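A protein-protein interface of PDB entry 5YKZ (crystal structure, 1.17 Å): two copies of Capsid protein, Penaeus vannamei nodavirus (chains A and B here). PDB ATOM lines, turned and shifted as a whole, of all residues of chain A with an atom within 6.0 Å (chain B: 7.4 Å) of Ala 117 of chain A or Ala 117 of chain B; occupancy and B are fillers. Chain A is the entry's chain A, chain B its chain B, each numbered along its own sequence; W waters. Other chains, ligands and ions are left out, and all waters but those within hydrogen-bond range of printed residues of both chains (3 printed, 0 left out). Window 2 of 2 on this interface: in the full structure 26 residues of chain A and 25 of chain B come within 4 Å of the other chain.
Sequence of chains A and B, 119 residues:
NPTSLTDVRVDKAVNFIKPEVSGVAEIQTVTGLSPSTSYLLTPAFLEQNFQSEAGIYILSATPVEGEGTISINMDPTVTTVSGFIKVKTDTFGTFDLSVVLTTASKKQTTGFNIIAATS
O of Arg 9 of chain B sits at hydrogen-bond distance from N of Ala 116 of chain B (2.9 Å).
O of Leu 40 of chain B sits at hydrogen-bond distance from N of Ile 115 of chain B, 2.8 Å away.
The backbone NH (N) of Thr 118 of chain B is in hydrogen-bond range of the backbone carbonyl oxygen (O) of Asp 7 of chain B.
The backbone carbonyl oxygen (O) of Asp 7 of chain A lies within hydrogen-bond range of the backbone NH (N) of Thr 118 of chain A.
NH2 of Arg 9 of chain A is in salt-bridge range of OD2 of Asp 7 of chain A (3.3 Å).
Asp 7 of chain A touches Ser 38 of chain B.
Asp 7 of chain A touches Ala 117 of chain B (O to CB, 3.95 Å).
Val 8 of chain A touches Ile 115 of chain B (CG1 to CG2, 3.8 Å).
Ala 116 of chain B touches Val 8 of chain A (C to CG2, 3.6 Å).
Val 8 of chain A touches Ala 117 of chain B.
OD2 of Asp 7 of chain B touches CB of Ser 38 of chain A, at 3.2 Å.
O of Ser 38 of chain A touches CG1 of Val 8 of chain B (3.9 Å).
Ile 115 of chain A touches Val 8 of chain B.
Ile 115 of chain A touches Ile 115 of chain B.
Asp 7 of chain B touches Ala 117 of chain A (O to CB, 3.3 Å).
Arg 9 of chain A touches none of the printed residues of chain B.
Thr 37 of chain A touches none of the printed residues of chain B.
Of the printed residues of chain B, Ser 38 of chain A touches Asp 7 (3.2 Å) and Val 8 (3.9 Å).
Of the printed residues of chain B, Ile 115 of chain A touches Val 8 (3.8 Å), Leu 40 (3.7 Å) and Ile 115 (3.8 Å).
Of chain B, only Asp 7 and Ala 117 come within 4 Å of Ala 117 of chain A.
Of the printed residues of chain A, Asp 7 of chain B touches Ser 38 and Ala 117.
Of the printed residues of chain A, Ser 38 of chain B touches Asp 7 (3.9 Å).
Of the printed residues of chain A, Ala 116 of chain B touches Val 8 (3.6 Å).
Of the printed residues of chain A, Ala 117 of chain B touches Asp 7 (3.95 Å), Val 8 (3.2 Å) and Ala 117 (3.7 Å).
Of the 14 printed residues of chain B, 7 touch a printed residue of chain A.
Hydrophobic or aromatic side chains of chain B within 4 Å of the printed part of chain A: Val 8, Leu 40, Ile 115 and Ala 117.
Among the printed residues, 12 pairs touch across the chains.
Among the printed residues, no Asp or Glu carboxylate lies within 4 Å of a Lys or Arg side-chain nitrogen of the other chain.
Asp 7 of chain A touches Ser 38 of chain B, and with the chains exchanged Ser 38 of chain A touches Asp 7 of chain B.
Asp 7 of chain A touches Ala 117 of chain B, and with the chains exchanged Ala 117 of chain A touches Asp 7 of chain B.
Ser 38 of chain A touches Val 8 of chain B, but with the chains exchanged Val 8 of chain A does not touch Ser 38 of chain B (4.7 Å).
Ile 115 of chain A touches its own counterpart, Ile 115 of chain B.
Of the 12 pairs that touch across the chains among the printed residues, 8 have their exchanged pair printed and touching as well.
Water W3 lies within hydrogen-bond range of O of Thr 6 of chain B (2.5 Å), O of Ser 38 of chain A (2.8 Å) and N of Ala 117 of chain A (3.0 Å).
Water W2 lies within hydrogen-bond range of the backbone carbonyl oxygen (O) of Thr 6 of chain B (2.6 Å) and the backbone NH (N) of Ser 38 of chain A (2.9 Å).
Water W1 bridges O of Ser 38 of chain B (3.3 Å) and N of Asp 7 of chain A (3.5 Å).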
ATOM      1  N   ASP A   7      18.567 -23.703  16.760  1.00  0.00           N
ATOM      2  CA  ASP A   7      18.047 -22.335  17.120  1.00  0.00           C
ATOM      3  C   ASP A   7      16.534 -22.255  16.875  1.00  0.00           C
ATOM      4  O   ASP A   7      15.954 -23.256  16.416  1.00  0.00           O
ATOM      5  CB  ASP A   7      18.795 -21.263  16.316  1.00  0.00           C
ATOM      6  CG  ASP A   7      18.780 -19.883  16.934  1.00  0.00           C
ATOM      7  OD1 ASP A   7      18.434 -19.748  18.123  1.00  0.00           O
ATOM      8  OD2 ASP A   7      19.057 -18.941  16.131  1.00  0.00           O
ATOM      9  N   VAL A   8      15.945 -21.140  17.300  1.00  0.00           N
ATOM     10  CA  VAL A   8      14.576 -20.747  16.957  1.00  0.00           C
ATOM     11  C   VAL A   8      14.614 -19.382  16.463  1.00  0.00           C
ATOM     12  O   VAL A   8      15.202 -18.515  17.150  1.00  0.00           O
ATOM     13  CB  VAL A   8      13.732 -20.765  18.279  1.00  0.00           C
ATOM     14  CG1 VAL A   8      12.316 -20.366  18.018  1.00  0.00           C
ATOM     15  CG2 VAL A   8      13.804 -22.118  18.907  1.00  0.00           C
ATOM     16  N   ARG A   9      13.970 -19.101  15.335  1.00  0.00           N
ATOM     17  CA  ARG A   9      13.987 -17.757  14.748  1.00  0.00           C
ATOM     18  C   ARG A   9      12.675 -17.381  14.160  1.00  0.00           C
ATOM     19  O   ARG A   9      11.934 -18.237  13.730  1.00  0.00           O
ATOM     20  CB  ARG A   9      15.035 -17.680  13.647  1.00  0.00           C
ATOM     21  CG  ARG A   9      16.419 -17.897  14.212  1.00  0.00           C
ATOM     22  CD  ARG A   9      17.475 -17.462  13.206  1.00  0.00           C
ATOM     23  NE  ARG A   9      17.488 -18.448  12.109  1.00  0.00           N
ATOM     24  CZ  ARG A   9      18.422 -19.425  11.969  1.00  0.00           C
ATOM     25  NH1 ARG A   9      18.456 -20.222  10.861  1.00  0.00           N
ATOM     26  NH2 ARG A   9      19.275 -19.677  12.953  1.00  0.00           N
ATOM     27  N   THR A  37       7.420 -28.091   6.778  1.00  0.00           N
ATOM     28  CA  THR A  37       8.117 -27.576   7.943  1.00  0.00           C
ATOM     29  C   THR A  37       7.103 -27.094   8.976  1.00  0.00           C
ATOM     30  O   THR A  37       6.107 -26.514   8.675  1.00  0.00           O
ATOM     31  CB  THR A  37       9.083 -26.466   7.525  1.00  0.00           C
ATOM     32  OG1 THR A  37      10.086 -27.005   6.670  1.00  0.00           O
ATOM     33  CG2 THR A  37       9.750 -25.714   8.694  1.00  0.00           C
ATOM     34  N   SER A  38       7.449 -27.365  10.210  1.00  0.00           N
ATOM     35  CA  SER A  38       6.617 -26.978  11.369  1.00  0.00           C
ATOM     36  C   SER A  38       6.907 -25.531  11.759  1.00  0.00           C
ATOM     37  O   SER A  38       8.066 -25.196  12.067  1.00  0.00           O
ATOM     38  CB  SER A  38       6.889 -27.898  12.543  1.00  0.00           C
ATOM     39  OG  SER A  38       6.315 -29.190  12.228  1.00  0.00           O
ATOM     40  N   ILE A 115       7.573 -18.617  13.255  1.00  0.00           N
ATOM     41  CA  ILE A 115       8.751 -19.102  13.932  1.00  0.00           C
ATOM     42  C   ILE A 115       9.044 -20.516  13.599  1.00  0.00           C
ATOM     43  O   ILE A 115       8.171 -21.342  13.587  1.00  0.00           O
ATOM     44  CB  ILE A 115       8.521 -18.918  15.459  1.00  0.00           C
ATOM     45  CG1 ILE A 115       8.352 -17.482  15.782  1.00  0.00           C
ATOM     46  CG2 ILE A 115       9.680 -19.516  16.243  1.00  0.00           C
ATOM     47  CD1 ILE A 115       7.590 -17.170  17.036  1.00  0.00           C
ATOM     48  N   ALA A 116      10.317 -20.783  13.308  1.00  0.00           N
ATOM     49  CA  ALA A 116      10.768 -22.142  13.029  1.00  0.00           C
ATOM     50  C   ALA A 116      12.082 -22.425  13.765  1.00  0.00           C
ATOM     51  O   ALA A 116      12.797 -21.523  14.150  1.00  0.00           O
ATOM     52  CB  ALA A 116      10.947 -22.426  11.539  1.00  0.00           C
ATOM     53  N   ALA A 117      12.335 -23.702  13.976  1.00  0.00           N
ATOM     54  CA  ALA A 117      13.628 -24.167  14.497  1.00  0.00           C
ATOM     55  C   ALA A 117      14.439 -24.640  13.380  1.00  0.00           C
ATOM     56  O   ALA A 117      13.959 -25.424  12.527  1.00  0.00           O
ATOM     57  CB  ALA A 117      13.405 -25.297  15.488  1.00  0.00           C
ATOM     58  N   THR A 118      15.705 -24.184  13.367  1.00  0.00           N
ATOM     59  CA  THR A 118      16.523 -24.410  12.102  1.00  0.00           C
ATOM     60  C   THR A 118      17.961 -24.692  12.380  1.00  0.00           C
ATOM     61  O   THR A 118      18.465 -24.283  13.437  1.00  0.00           O
ATOM     62  CB  THR A 118      16.305 -23.302  11.021  1.00  0.00           C
ATOM     63  OG1 THR A 118      17.429 -23.278  10.079  1.00  0.00           O
ATOM     64  CG2 THR A 118      16.021 -21.912  11.681  1.00  0.00           C
ATOM     65  N   THR B   6      14.064 -29.808  14.640  1.00  0.00           N
ATOM     66  CA  THR B   6      13.075 -29.680  13.530  1.00  0.00           C
ATOM     67  C   THR B   6      11.720 -29.060  13.822  1.00  0.00           C
ATOM     68  O   THR B   6      11.161 -28.301  12.950  1.00  0.00           O
ATOM     69  CB  THR B   6      12.991 -31.010  12.682  1.00  0.00           C
ATOM     70  OG1 THR B   6      13.166 -32.243  13.511  1.00  0.00           O
ATOM     71  CG2 THR B   6      14.048 -30.953  11.572  1.00  0.00           C
ATOM     72  N   ASP B   7      11.275 -29.168  15.065  1.00  0.00           N
ATOM     73  CA  ASP B   7       9.939 -28.695  15.504  1.00  0.00           C
ATOM     74  C   ASP B   7      10.176 -27.594  16.579  1.00  0.00           C
ATOM     75  O   ASP B   7      11.288 -27.355  16.987  1.00  0.00           O
ATOM     76  CB  ASP B   7       9.080 -29.865  16.023  1.00  0.00           C
ATOM     77  CG  ASP B   7       7.604 -29.555  16.114  1.00  0.00           C
ATOM     78  OD1 ASP B   7       6.889 -30.484  16.682  1.00  0.00           O
ATOM     79  OD2 ASP B   7       7.083 -28.546  15.680  1.00  0.00           O
ATOM     80  N   VAL B   8       9.112 -26.888  16.879  1.00  0.00           N
ATOM     81  CA  VAL B   8       9.117 -25.763  17.788  1.00  0.00           C
ATOM     82  C   VAL B   8       7.938 -25.863  18.689  1.00  0.00           C
ATOM     83  O   VAL B   8       6.884 -26.274  18.272  1.00  0.00           O
ATOM     84  CB  VAL B   8       9.186 -24.505  16.916  1.00  0.00           C
ATOM     85  CG1 VAL B   8       8.168 -24.387  15.853  1.00  0.00           C
ATOM     86  CG2 VAL B   8       9.053 -23.303  17.753  1.00  0.00           C
ATOM     87  N   ARG B   9       8.090 -25.468  19.935  1.00  0.00           N
ATOM     88  CA  ARG B   9       7.007 -25.494  20.861  1.00  0.00           C
ATOM     89  C   ARG B   9       7.129 -24.382  21.863  1.00  0.00           C
ATOM     90  O   ARG B   9       8.203 -23.805  22.018  1.00  0.00           O
ATOM     91  CB  ARG B   9       7.006 -26.857  21.572  1.00  0.00           C
ATOM     92  CG  ARG B   9       8.207 -27.128  22.411  1.00  0.00           C
ATOM     93  CD  ARG B   9       8.161 -28.521  23.132  1.00  0.00           C
ATOM     94  NE  ARG B   9       8.741 -28.407  24.439  1.00  0.00           N
ATOM     95  CZ  ARG B   9       8.038 -28.266  25.582  1.00  0.00           C
ATOM     96  NH1 ARG B   9       6.684 -28.239  25.608  1.00  0.00           N
ATOM     97  NH2 ARG B   9       8.714 -28.152  26.702  1.00  0.00           N
ATOM     98  N   ASP B  11       7.682 -23.906  25.397  1.00  0.00           N
ATOM     99  CA  ASP B  11       8.188 -24.602  26.546  1.00  0.00           C
ATOM    100  C   ASP B  11       7.526 -24.256  27.840  1.00  0.00           C
ATOM    101  O   ASP B  11       7.190 -25.142  28.719  1.00  0.00           O
ATOM    102  CB  ASP B  11       9.665 -24.430  26.691  1.00  0.00           C
ATOM    103  CG  ASP B  11      10.152 -25.177  27.902  1.00  0.00           C
ATOM    104  OD1 ASP B  11      10.220 -26.401  27.821  1.00  0.00           O
ATOM    105  OD2 ASP B  11      10.277 -24.584  28.995  1.00  0.00           O
ATOM    106  N   THR B  37      21.284 -22.823  26.291  1.00  0.00           N
ATOM    107  CA  THR B  37      20.356 -23.023  25.198  1.00  0.00           C
ATOM    108  C   THR B  37      19.650 -21.667  24.900  1.00  0.00           C
ATOM    109  O   THR B  37      19.319 -20.930  25.822  1.00  0.00           O
ATOM    110  CB  THR B  37      19.264 -24.026  25.598  1.00  0.00           C
ATOM    111  OG1 THR B  37      19.935 -25.318  25.887  1.00  0.00           O
ATOM    112  CG2 THR B  37      18.262 -24.316  24.483  1.00  0.00           C
ATOM    113  N   SER B  38      19.409 -21.469  23.641  1.00  0.00           N
ATOM    114  CA  SER B  38      18.737 -20.230  23.166  1.00  0.00           C
ATOM    115  C   SER B  38      17.269 -20.472  23.007  1.00  0.00           C
ATOM    116  O   SER B  38      16.762 -21.497  22.536  1.00  0.00           O
ATOM    117  CB  SER B  38      19.390 -19.787  21.888  1.00  0.00           C
ATOM    118  OG  SER B  38      20.728 -19.254  22.262  1.00  0.00           O
ATOM    119  N   TYR B  39      16.539 -19.412  23.405  1.00  0.00           N
ATOM    120  CA  TYR B  39      15.060 -19.353  23.374  1.00  0.00           C
ATOM    121  C   TYR B  39      14.594 -18.108  22.730  1.00  0.00           C
ATOM    122  O   TYR B  39      15.332 -17.070  22.787  1.00  0.00           O
ATOM    123  CB  TYR B  39      14.503 -19.467  24.801  1.00  0.00           C
ATOM    124  CG  TYR B  39      14.837 -20.743  25.457  1.00  0.00           C
ATOM    125  CD1 TYR B  39      14.011 -21.848  25.285  1.00  0.00           C
ATOM    126  CD2 TYR B  39      15.962 -20.917  26.254  1.00  0.00           C
ATOM    127  CE1 TYR B  39      14.331 -23.078  25.850  1.00  0.00           C
ATOM    128  CE2 TYR B  39      16.259 -22.149  26.836  1.00  0.00           C
ATOM    129  CZ  TYR B  39      15.427 -23.187  26.606  1.00  0.00           C
ATOM    130  OH  TYR B  39      15.737 -24.407  27.240  1.00  0.00           O
ATOM    131  N   LEU B  40      13.417 -18.081  22.221  1.00  0.00           N
ATOM    132  CA  LEU B  40      12.726 -16.837  21.756  1.00  0.00           C
ATOM    133  C   LEU B  40      11.604 -16.541  22.712  1.00  0.00           C
ATOM    134  O   LEU B  40      10.850 -17.479  23.088  1.00  0.00           O
ATOM    135  CB  LEU B  40      12.193 -17.136  20.404  1.00  0.00           C
ATOM    136  CG  LEU B  40      11.756 -15.997  19.594  1.00  0.00           C
ATOM    137  CD1 LEU B  40      12.926 -15.073  19.116  1.00  0.00           C
ATOM    138  CD2 LEU B  40      10.915 -16.448  18.407  1.00  0.00           C
ATOM    139  N   ILE B 115       9.781 -19.994  23.764  1.00  0.00           N
ATOM    140  CA  ILE B 115       9.689 -20.831  22.558  1.00  0.00           C
ATOM    141  C   ILE B 115      11.029 -21.475  22.344  1.00  0.00           C
ATOM    142  O   ILE B 115      12.066 -20.886  22.451  1.00  0.00           O
ATOM    143  CB  ILE B 115       9.316 -19.999  21.352  1.00  0.00           C
ATOM    144  CG1 ILE B 115       8.009 -19.298  21.623  1.00  0.00           C
ATOM    145  CG2 ILE B 115       9.197 -20.894  20.133  1.00  0.00           C
ATOM    146  CD1 ILE B 115       7.663 -18.218  20.736  1.00  0.00           C
ATOM    147  N   ALA B 116      10.950 -22.814  22.130  1.00  0.00           N
ATOM    148  CA  ALA B 116      12.097 -23.701  22.082  1.00  0.00           C
ATOM    149  C   ALA B 116      12.045 -24.610  20.860  1.00  0.00           C
ATOM    150  O   ALA B 116      10.963 -25.076  20.486  1.00  0.00           O
ATOM    151  CB  ALA B 116      12.099 -24.571  23.364  1.00  0.00           C
ATOM    152  N   ALA B 117      13.216 -24.942  20.387  1.00  0.00           N
ATOM    153  CA  ALA B 117      13.296 -26.046  19.476  1.00  0.00           C
ATOM    154  C   ALA B 117      13.079 -27.370  20.173  1.00  0.00           C
ATOM    155  O   ALA B 117      13.466 -27.549  21.309  1.00  0.00           O
ATOM    156  CB  ALA B 117      14.672 -26.067  18.883  1.00  0.00           C
ATOM    157  N   THR B 118      12.494 -28.299  19.445  1.00  0.00           N
ATOM    158  CA  THR B 118      12.266 -29.681  19.878  1.00  0.00           C
ATOM    159  C   THR B 118      12.276 -30.589  18.644  1.00  0.00           C
ATOM    160  O   THR B 118      12.452 -30.154  17.525  1.00  0.00           O
ATOM    161  CB  THR B 118      10.902 -29.723  20.579  1.00  0.00           C
ATOM    162  OG1 THR B 118      10.680 -30.996  21.249  1.00  0.00           O
ATOM    163  CG2 THR B 118       9.702 -29.459  19.676  1.00  0.00           C
ATOM    164  N   SER B 119      12.151 -31.882  18.899  1.00  0.00           N
ATOM    165  CA  SER B 119      11.999 -32.904  17.823  1.00  0.00           C
ATOM    166  C   SER B 119      10.605 -32.933  17.226  1.00  0.00           C
ATOM    167  O   SER B 119      10.497 -33.473  16.123  1.00  0.00           O
ATOM    168  CB  SER B 119      12.238 -34.251  18.447  1.00  0.00           C
ATOM    169  OG  SER B 119      11.343 -34.415  19.529  1.00  0.00           O
HETATM  170  O   HOH W   1      17.283 -23.497  20.005  1.00  0.00           O
HETATM  171  O   HOH W   2       9.897 -28.878  10.712  1.00  0.00           O
HETATM  172  O   HOH W   3      10.522 -25.904  13.164  1.00  0.00           O
